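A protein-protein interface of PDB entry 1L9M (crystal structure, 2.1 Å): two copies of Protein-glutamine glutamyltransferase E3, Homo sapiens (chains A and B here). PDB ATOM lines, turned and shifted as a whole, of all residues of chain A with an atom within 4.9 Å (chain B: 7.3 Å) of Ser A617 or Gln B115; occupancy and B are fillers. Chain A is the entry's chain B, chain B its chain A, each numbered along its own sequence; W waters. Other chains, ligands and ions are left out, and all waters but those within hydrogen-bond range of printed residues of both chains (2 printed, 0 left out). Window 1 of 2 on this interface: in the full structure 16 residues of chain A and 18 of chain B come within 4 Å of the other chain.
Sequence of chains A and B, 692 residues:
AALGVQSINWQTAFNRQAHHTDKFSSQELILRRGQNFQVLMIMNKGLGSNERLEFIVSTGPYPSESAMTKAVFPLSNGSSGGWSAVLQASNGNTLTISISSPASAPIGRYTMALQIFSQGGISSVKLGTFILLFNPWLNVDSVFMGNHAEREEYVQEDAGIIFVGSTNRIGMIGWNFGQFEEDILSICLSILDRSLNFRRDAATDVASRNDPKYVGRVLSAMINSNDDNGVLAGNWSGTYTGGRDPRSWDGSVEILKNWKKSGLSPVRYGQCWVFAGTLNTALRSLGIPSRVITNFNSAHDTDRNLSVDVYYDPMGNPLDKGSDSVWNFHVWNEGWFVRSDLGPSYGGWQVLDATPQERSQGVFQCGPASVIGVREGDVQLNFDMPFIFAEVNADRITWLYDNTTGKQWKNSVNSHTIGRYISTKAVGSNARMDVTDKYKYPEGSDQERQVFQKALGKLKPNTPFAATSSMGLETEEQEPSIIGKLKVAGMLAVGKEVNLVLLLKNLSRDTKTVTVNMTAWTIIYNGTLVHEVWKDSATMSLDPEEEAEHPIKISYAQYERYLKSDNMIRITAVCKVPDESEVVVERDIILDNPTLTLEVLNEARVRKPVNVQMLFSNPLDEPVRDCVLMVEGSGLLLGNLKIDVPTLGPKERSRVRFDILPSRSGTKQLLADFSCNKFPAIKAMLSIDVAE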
ATOM      1  N   PRO A 594      34.361 -20.026  10.591  1.00  0.00           N
ATOM      2  CA  PRO A 594      33.580 -19.650  11.776  1.00  0.00           C
ATOM      3  C   PRO A 594      32.357 -20.555  11.776  1.00  0.00           C
ATOM      4  O   PRO A 594      31.981 -21.080  10.728  1.00  0.00           O
ATOM      5  CB  PRO A 594      33.201 -18.200  11.500  1.00  0.00           C
ATOM      6  CG  PRO A 594      34.309 -17.713  10.619  1.00  0.00           C
ATOM      7  CD  PRO A 594      34.536 -18.876   9.688  1.00  0.00           C
ATOM      8  N   THR A 595      31.735 -20.743  12.930  1.00  0.00           N
ATOM      9  CA  THR A 595      30.569 -21.605  12.995  1.00  0.00           C
ATOM     10  C   THR A 595      29.395 -21.070  12.184  1.00  0.00           C
ATOM     11  O   THR A 595      29.174 -19.862  12.093  1.00  0.00           O
ATOM     12  CB  THR A 595      30.103 -21.814  14.454  1.00  0.00           C
ATOM     13  OG1 THR A 595      31.112 -22.526  15.182  1.00  0.00           O
ATOM     14  CG2 THR A 595      28.811 -22.624  14.490  1.00  0.00           C
ATOM     15  N   LEU A 615      22.133 -19.119  11.744  1.00  0.00           N
ATOM     16  CA  LEU A 615      22.901 -18.399  12.755  1.00  0.00           C
ATOM     17  C   LEU A 615      24.396 -18.318  12.441  1.00  0.00           C
ATOM     18  O   LEU A 615      25.066 -19.343  12.292  1.00  0.00           O
ATOM     19  CB  LEU A 615      22.713 -19.062  14.119  1.00  0.00           C
ATOM     20  CG  LEU A 615      21.277 -19.225  14.623  1.00  0.00           C
ATOM     21  CD1 LEU A 615      21.277 -20.054  15.898  1.00  0.00           C
ATOM     22  CD2 LEU A 615      20.654 -17.853  14.856  1.00  0.00           C
ATOM     23  N   PHE A 616      24.913 -17.094  12.354  1.00  0.00           N
ATOM     24  CA  PHE A 616      26.330 -16.866  12.075  1.00  0.00           C
ATOM     25  C   PHE A 616      26.844 -15.590  12.738  1.00  0.00           C
ATOM     26  O   PHE A 616      26.142 -14.581  12.793  1.00  0.00           O
ATOM     27  CB  PHE A 616      26.571 -16.754  10.568  1.00  0.00           C
ATOM     28  CG  PHE A 616      28.002 -16.427  10.203  1.00  0.00           C
ATOM     29  CD1 PHE A 616      28.982 -17.413  10.219  1.00  0.00           C
ATOM     30  CD2 PHE A 616      28.370 -15.124   9.868  1.00  0.00           C
ATOM     31  CE1 PHE A 616      30.310 -17.112   9.907  1.00  0.00           C
ATOM     32  CE2 PHE A 616      29.696 -14.811   9.555  1.00  0.00           C
ATOM     33  CZ  PHE A 616      30.668 -15.810   9.574  1.00  0.00           C
ATOM     34  N   SER A 617      28.078 -15.641  13.232  1.00  0.00           N
ATOM     35  CA  SER A 617      28.707 -14.484  13.856  1.00  0.00           C
ATOM     36  C   SER A 617      30.070 -14.206  13.208  1.00  0.00           C
ATOM     37  O   SER A 617      30.893 -15.112  13.067  1.00  0.00           O
ATOM     38  CB  SER A 617      28.879 -14.717  15.362  1.00  0.00           C
ATOM     39  OG  SER A 617      27.661 -14.505  16.059  1.00  0.00           O
ATOM     40  N   ASN A 618      30.297 -12.955  12.812  1.00  0.00           N
ATOM     41  CA  ASN A 618      31.559 -12.549  12.183  1.00  0.00           C
ATOM     42  C   ASN A 618      32.626 -12.340  13.249  1.00  0.00           C
ATOM     43  O   ASN A 618      32.531 -11.424  14.061  1.00  0.00           O
ATOM     44  CB  ASN A 618      31.358 -11.259  11.378  1.00  0.00           C
ATOM     45  CG  ASN A 618      32.661 -10.705  10.794  1.00  0.00           C
ATOM     46  OD1 ASN A 618      33.714 -11.349  10.838  1.00  0.00           O
ATOM     47  ND2 ASN A 618      32.582  -9.500  10.237  1.00  0.00           N
ATOM     48  N   PRO A 619      33.663 -13.188  13.255  1.00  0.00           N
ATOM     49  CA  PRO A 619      34.748 -13.090  14.236  1.00  0.00           C
ATOM     50  C   PRO A 619      35.813 -12.047  13.901  1.00  0.00           C
ATOM     51  O   PRO A 619      36.678 -11.757  14.728  1.00  0.00           O
ATOM     52  CB  PRO A 619      35.323 -14.498  14.240  1.00  0.00           C
ATOM     53  CG  PRO A 619      35.237 -14.860  12.773  1.00  0.00           C
ATOM     54  CD  PRO A 619      33.851 -14.361  12.378  1.00  0.00           C
ATOM     55  N   GLU A 652      29.667  -8.919  14.820  1.00  0.00           N
ATOM     56  CA  GLU A 652      28.227  -8.845  14.603  1.00  0.00           C
ATOM     57  C   GLU A 652      27.605 -10.203  14.265  1.00  0.00           C
ATOM     58  O   GLU A 652      28.296 -11.138  13.858  1.00  0.00           O
ATOM     59  CB  GLU A 652      27.974  -7.846  13.483  1.00  0.00           C
ATOM     60  CG  GLU A 652      26.606  -7.238  13.413  1.00  0.00           C
ATOM     61  CD  GLU A 652      26.660  -5.890  12.718  1.00  0.00           C
ATOM     62  OE1 GLU A 652      27.251  -4.951  13.303  1.00  0.00           O
ATOM     63  OE2 GLU A 652      26.134  -5.774  11.588  1.00  0.00           O
ATOM     64  N   ARG A 653      26.291 -10.299  14.432  1.00  0.00           N
ATOM     65  CA  ARG A 653      25.566 -11.536  14.171  1.00  0.00           C
ATOM     66  C   ARG A 653      24.539 -11.372  13.058  1.00  0.00           C
ATOM     67  O   ARG A 653      23.952 -10.303  12.885  1.00  0.00           O
ATOM     68  CB  ARG A 653      24.875 -11.996  15.453  1.00  0.00           C
ATOM     69  CG  ARG A 653      23.665 -12.888  15.257  1.00  0.00           C
ATOM     70  CD  ARG A 653      22.721 -12.696  16.431  1.00  0.00           C
ATOM     71  NE  ARG A 653      22.768 -11.306  16.879  1.00  0.00           N
ATOM     72  CZ  ARG A 653      21.915 -10.751  17.732  1.00  0.00           C
ATOM     73  NH1 ARG A 653      20.926 -11.467  18.241  1.00  0.00           N
ATOM     74  NH2 ARG A 653      22.061  -9.480  18.086  1.00  0.00           N
ATOM     75  N   ARG B  52      34.828  -8.884  23.185  1.00  0.00           N
ATOM     76  CA  ARG B  52      33.411  -8.656  23.433  1.00  0.00           C
ATOM     77  C   ARG B  52      32.689  -9.865  24.012  1.00  0.00           C
ATOM     78  O   ARG B  52      32.992 -11.015  23.678  1.00  0.00           O
ATOM     79  CB  ARG B  52      32.678  -8.237  22.155  1.00  0.00           C
ATOM     80  CG  ARG B  52      31.185  -8.075  22.411  1.00  0.00           C
ATOM     81  CD  ARG B  52      30.332  -8.053  21.158  1.00  0.00           C
ATOM     82  NE  ARG B  52      30.475  -6.822  20.390  1.00  0.00           N
ATOM     83  CZ  ARG B  52      29.607  -6.428  19.463  1.00  0.00           C
ATOM     84  NH1 ARG B  52      28.538  -7.170  19.199  1.00  0.00           N
ATOM     85  NH2 ARG B  52      29.811  -5.299  18.796  1.00  0.00           N
ATOM     86  N   LEU B  53      31.720  -9.585  24.875  1.00  0.00           N
ATOM     87  CA  LEU B  53      30.914 -10.623  25.498  1.00  0.00           C
ATOM     88  C   LEU B  53      29.456 -10.394  25.121  1.00  0.00           C
ATOM     89  O   LEU B  53      28.946  -9.285  25.258  1.00  0.00           O
ATOM     90  CB  LEU B  53      31.047 -10.572  27.020  1.00  0.00           C
ATOM     91  CG  LEU B  53      32.443 -10.623  27.644  1.00  0.00           C
ATOM     92  CD1 LEU B  53      32.311 -10.645  29.158  1.00  0.00           C
ATOM     93  CD2 LEU B  53      33.184 -11.847  27.167  1.00  0.00           C
ATOM     94  N   GLU B  54      28.793 -11.433  24.625  1.00  0.00           N
ATOM     95  CA  GLU B  54      27.380 -11.320  24.279  1.00  0.00           C
ATOM     96  C   GLU B  54      26.610 -12.390  25.034  1.00  0.00           C
ATOM     97  O   GLU B  54      26.938 -13.573  24.967  1.00  0.00           O
ATOM     98  CB  GLU B  54      27.147 -11.485  22.774  1.00  0.00           C
ATOM     99  CG  GLU B  54      27.771 -10.384  21.927  1.00  0.00           C
ATOM    100  CD  GLU B  54      26.843  -9.880  20.833  1.00  0.00           C
ATOM    101  OE1 GLU B  54      25.759  -9.354  21.168  1.00  0.00           O
ATOM    102  OE2 GLU B  54      27.195 -10.007  19.641  1.00  0.00           O
ATOM    103  N   PHE B  55      25.593 -11.963  25.770  1.00  0.00           N
ATOM    104  CA  PHE B  55      24.779 -12.889  26.533  1.00  0.00           C
ATOM    105  C   PHE B  55      23.668 -13.445  25.666  1.00  0.00           C
ATOM    106  O   PHE B  55      23.164 -12.776  24.764  1.00  0.00           O
ATOM    107  CB  PHE B  55      24.180 -12.195  27.765  1.00  0.00           C
ATOM    108  CG  PHE B  55      25.205 -11.793  28.789  1.00  0.00           C
ATOM    109  CD1 PHE B  55      26.031 -10.699  28.574  1.00  0.00           C
ATOM    110  CD2 PHE B  55      25.365 -12.534  29.954  1.00  0.00           C
ATOM    111  CE1 PHE B  55      27.003 -10.350  29.502  1.00  0.00           C
ATOM    112  CE2 PHE B  55      26.334 -12.193  30.887  1.00  0.00           C
ATOM    113  CZ  PHE B  55      27.155 -11.100  30.662  1.00  0.00           C
ATOM    114  N   ILE B  56      23.297 -14.685  25.946  1.00  0.00           N
ATOM    115  CA  ILE B  56      22.242 -15.343  25.206  1.00  0.00           C
ATOM    116  C   ILE B  56      21.332 -16.081  26.171  1.00  0.00           C
ATOM    117  O   ILE B  56      21.769 -16.974  26.897  1.00  0.00           O
ATOM    118  CB  ILE B  56      22.808 -16.361  24.214  1.00  0.00           C
ATOM    119  CG1 ILE B  56      23.892 -15.706  23.363  1.00  0.00           C
ATOM    120  CG2 ILE B  56      21.688 -16.897  23.334  1.00  0.00           C
ATOM    121  CD1 ILE B  56      24.559 -16.659  22.395  1.00  0.00           C
ATOM    122  N   VAL B  72      19.770 -11.932  22.488  1.00  0.00           N
ATOM    123  CA  VAL B  72      21.218 -11.810  22.420  1.00  0.00           C
ATOM    124  C   VAL B  72      21.542 -10.350  22.718  1.00  0.00           C
ATOM    125  O   VAL B  72      21.049  -9.448  22.043  1.00  0.00           O
ATOM    126  CB  VAL B  72      21.745 -12.168  21.015  1.00  0.00           C
ATOM    127  CG1 VAL B  72      23.267 -12.157  21.016  1.00  0.00           C
ATOM    128  CG2 VAL B  72      21.211 -13.530  20.586  1.00  0.00           C
ATOM    129  N   ALA B 113      23.698 -18.451  28.103  1.00  0.00           N
ATOM    130  CA  ALA B 113      24.997 -18.814  27.573  1.00  0.00           C
ATOM    131  C   ALA B 113      25.753 -17.523  27.295  1.00  0.00           C
ATOM    132  O   ALA B 113      25.159 -16.447  27.225  1.00  0.00           O
ATOM    133  CB  ALA B 113      24.835 -19.630  26.289  1.00  0.00           C
ATOM    134  N   LEU B 114      27.066 -17.625  27.149  1.00  0.00           N
ATOM    135  CA  LEU B 114      27.879 -16.451  26.873  1.00  0.00           C
ATOM    136  C   LEU B 114      28.757 -16.665  25.648  1.00  0.00           C
ATOM    137  O   LEU B 114      29.446 -17.672  25.538  1.00  0.00           O
ATOM    138  CB  LEU B 114      28.766 -16.134  28.075  1.00  0.00           C
ATOM    139  CG  LEU B 114      29.716 -14.954  27.883  1.00  0.00           C
ATOM    140  CD1 LEU B 114      28.916 -13.655  27.809  1.00  0.00           C
ATOM    141  CD2 LEU B 114      30.699 -14.905  29.034  1.00  0.00           C
ATOM    142  N   GLN B 115      28.728 -15.720  24.720  1.00  0.00           N
ATOM    143  CA  GLN B 115      29.563 -15.838  23.539  1.00  0.00           C
ATOM    144  C   GLN B 115      30.726 -14.875  23.726  1.00  0.00           C
ATOM    145  O   GLN B 115      30.528 -13.716  24.095  1.00  0.00           O
ATOM    146  CB  GLN B 115      28.772 -15.499  22.277  1.00  0.00           C
ATOM    147  CG  GLN B 115      29.391 -16.090  21.020  1.00  0.00           C
ATOM    148  CD  GLN B 115      28.546 -15.891  19.778  1.00  0.00           C
ATOM    149  OE1 GLN B 115      28.881 -16.392  18.706  1.00  0.00           O
ATOM    150  NE2 GLN B 115      27.451 -15.158  19.913  1.00  0.00           N
ATOM    151  N   ILE B 116      31.939 -15.358  23.488  1.00  0.00           N
ATOM    152  CA  ILE B 116      33.123 -14.534  23.665  1.00  0.00           C
ATOM    153  C   ILE B 116      33.926 -14.299  22.391  1.00  0.00           C
ATOM    154  O   ILE B 116      34.394 -15.243  21.749  1.00  0.00           O
ATOM    155  CB  ILE B 116      34.062 -15.143  24.729  1.00  0.00           C
ATOM    156  CG1 ILE B 116      33.347 -15.201  26.079  1.00  0.00           C
ATOM    157  CG2 ILE B 116      35.332 -14.310  24.850  1.00  0.00           C
ATOM    158  CD1 ILE B 116      34.153 -15.879  27.167  1.00  0.00           C
ATOM    159  N   PHE B 117      34.078 -13.029  22.037  1.00  0.00           N
ATOM    160  CA  PHE B 117      34.841 -12.639  20.866  1.00  0.00           C
ATOM    161  C   PHE B 117      36.224 -12.246  21.373  1.00  0.00           C
ATOM    162  O   PHE B 117      36.382 -11.226  22.047  1.00  0.00           O
ATOM    163  CB  PHE B 117      34.157 -11.466  20.171  1.00  0.00           C
ATOM    164  CG  PHE B 117      32.837 -11.827  19.552  1.00  0.00           C
ATOM    165  CD1 PHE B 117      32.759 -12.211  18.216  1.00  0.00           C
ATOM    166  CD2 PHE B 117      31.673 -11.817  20.314  1.00  0.00           C
ATOM    167  CE1 PHE B 117      31.543 -12.583  17.647  1.00  0.00           C
ATOM    168  CE2 PHE B 117      30.450 -12.188  19.758  1.00  0.00           C
ATOM    169  CZ  PHE B 117      30.384 -12.572  18.420  1.00  0.00           C
ATOM    170  N   SER B 118      37.220 -13.071  21.063  1.00  0.00           N
ATOM    171  CA  SER B 118      38.578 -12.823  21.521  1.00  0.00           C
ATOM    172  C   SER B 118      39.631 -13.422  20.587  1.00  0.00           C
ATOM    173  O   SER B 118      39.472 -14.533  20.080  1.00  0.00           O
ATOM    174  CB  SER B 118      38.742 -13.405  22.928  1.00  0.00           C
ATOM    175  OG  SER B 118      40.031 -13.159  23.456  1.00  0.00           O
ATOM    176  N   ILE B 122      35.871 -16.972  18.151  1.00  0.00           N
ATOM    177  CA  ILE B 122      34.614 -16.918  18.889  1.00  0.00           C
ATOM    178  C   ILE B 122      34.441 -18.195  19.695  1.00  0.00           C
ATOM    179  O   ILE B 122      34.661 -19.289  19.178  1.00  0.00           O
ATOM    180  CB  ILE B 122      33.389 -16.803  17.952  1.00  0.00           C
ATOM    181  CG1 ILE B 122      33.532 -15.588  17.032  1.00  0.00           C
ATOM    182  CG2 ILE B 122      32.114 -16.681  18.786  1.00  0.00           C
ATOM    183  CD1 ILE B 122      32.396 -15.440  16.032  1.00  0.00           C
ATOM    184  N   SER B 123      34.058 -18.056  20.959  1.00  0.00           N
ATOM    185  CA  SER B 123      33.835 -19.212  21.817  1.00  0.00           C
ATOM    186  C   SER B 123      32.478 -19.058  22.503  1.00  0.00           C
ATOM    187  O   SER B 123      31.966 -17.946  22.643  1.00  0.00           O
ATOM    188  CB  SER B 123      34.945 -19.333  22.864  1.00  0.00           C
ATOM    189  OG  SER B 123      34.846 -18.312  23.836  1.00  0.00           O
ATOM    190  N   SER B 124      31.894 -20.172  22.931  1.00  0.00           N
ATOM    191  CA  SER B 124      30.592 -20.132  23.582  1.00  0.00           C
ATOM    192  C   SER B 124      30.534 -21.103  24.752  1.00  0.00           C
ATOM    193  O   SER B 124      30.923 -22.265  24.620  1.00  0.00           O
ATOM    194  CB  SER B 124      29.501 -20.473  22.567  1.00  0.00           C
ATOM    195  OG  SER B 124      28.231 -20.062  23.034  1.00  0.00           O
ATOM    196  N   VAL B 125      30.054 -20.623  25.896  1.00  0.00           N
ATOM    197  CA  VAL B 125      29.950 -21.458  27.087  1.00  0.00           C
ATOM    198  C   VAL B 125      28.615 -21.233  27.781  1.00  0.00           C
ATOM    199  O   VAL B 125      28.108 -20.112  27.814  1.00  0.00           O
ATOM    200  CB  VAL B 125      31.084 -21.149  28.089  1.00  0.00           C
ATOM    201  CG1 VAL B 125      30.990 -19.712  28.555  1.00  0.00           C
ATOM    202  CG2 VAL B 125      31.004 -22.093  29.273  1.00  0.00           C
ATOM    203  N   LEU B 127      26.372 -20.607  30.837  1.00  0.00           N
ATOM    204  CA  LEU B 127      26.539 -20.046  32.173  1.00  0.00           C
ATOM    205  C   LEU B 127      25.647 -20.712  33.214  1.00  0.00           C
ATOM    206  O   LEU B 127      26.051 -20.885  34.360  1.00  0.00           O
ATOM    207  CB  LEU B 127      26.257 -18.546  32.144  1.00  0.00           C
ATOM    208  CG  LEU B 127      27.211 -17.741  31.264  1.00  0.00           C
ATOM    209  CD1 LEU B 127      26.695 -16.329  31.111  1.00  0.00           C
ATOM    210  CD2 LEU B 127      28.606 -17.752  31.876  1.00  0.00           C
HETATM  211  O   HOH W   1      26.611 -12.974  17.755  1.00  0.00           O
HETATM  212  O   HOH W   2      23.452  -8.315  20.465  1.00  0.00           O
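The side-chain amide oxygen of Gln B115 lies within hydrogen-bond range of the side-chain hydroxyl of Ser A617.
N of Phe B117 is in hydrogen-bond range of O of Arg B52, 2.8 Å away.
N of Gln B115 is in hydrogen-bond range of O of Glu B54 (2.8 Å).
N of Asn A618 is in hydrogen-bond range of O of Glu A652 (2.9 Å).
O of Ser A617 touches CD1 of Ile B122, at 3.3 Å.
CE1 of Phe B117 touches O of Asn A618 (3.9 Å).
CB of Pro A619 touches CG1 of Ile B122, at 3.5 Å.
NH1 of Arg A653 touches CB of Val B72, 3.0 Å away.
Of the printed residues of chain B, Asn A618 touches Phe B117.
Of the printed residues of chain A, Val B72 touches Arg A653 (3.0 Å).
Gln B115 touches one residue of chain A.
Of the printed residues of chain A, Phe B117 touches Asn A618.
Of the printed residues of chain A, Ile B122 touches Ser A617 and Pro A619.
The nearest residue of chain B that does not touch Ser A617 is Phe B117 (4.03 Å).
The nearest printed residue of chain A that does not touch Gln B115 is Arg A653 (6.0 Å).
The nearest printed residue of chain A that does not touch Phe B117 is Ser A617 (4.03 Å).
Of the 17 printed residues of chain B, 4 touch a printed residue of chain A.
Printed residues of chain A that touch a printed residue of chain B: Ser A617, Asn A618, Pro A619 and Arg A653.
Hydrophobic or aromatic side chains of chain A that line the printed part of chain B: Pro A619.
No position is printed for both chains.
Of the 5 pairs that touch across the chains among the printed residues, none has its exchanged pair printed and touching as well.
Water W1 lies within hydrogen-bond range of OG of Ser A617 and NE2 of Gln B115.
Water W2 lies within hydrogen-bond range of the side-chain carboxylate of Glu B54 (2.6 Å), the guanidinium group of Arg A653 (3.0 Å) and the backbone carbonyl oxygen of Val B72 (3.1 Å).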
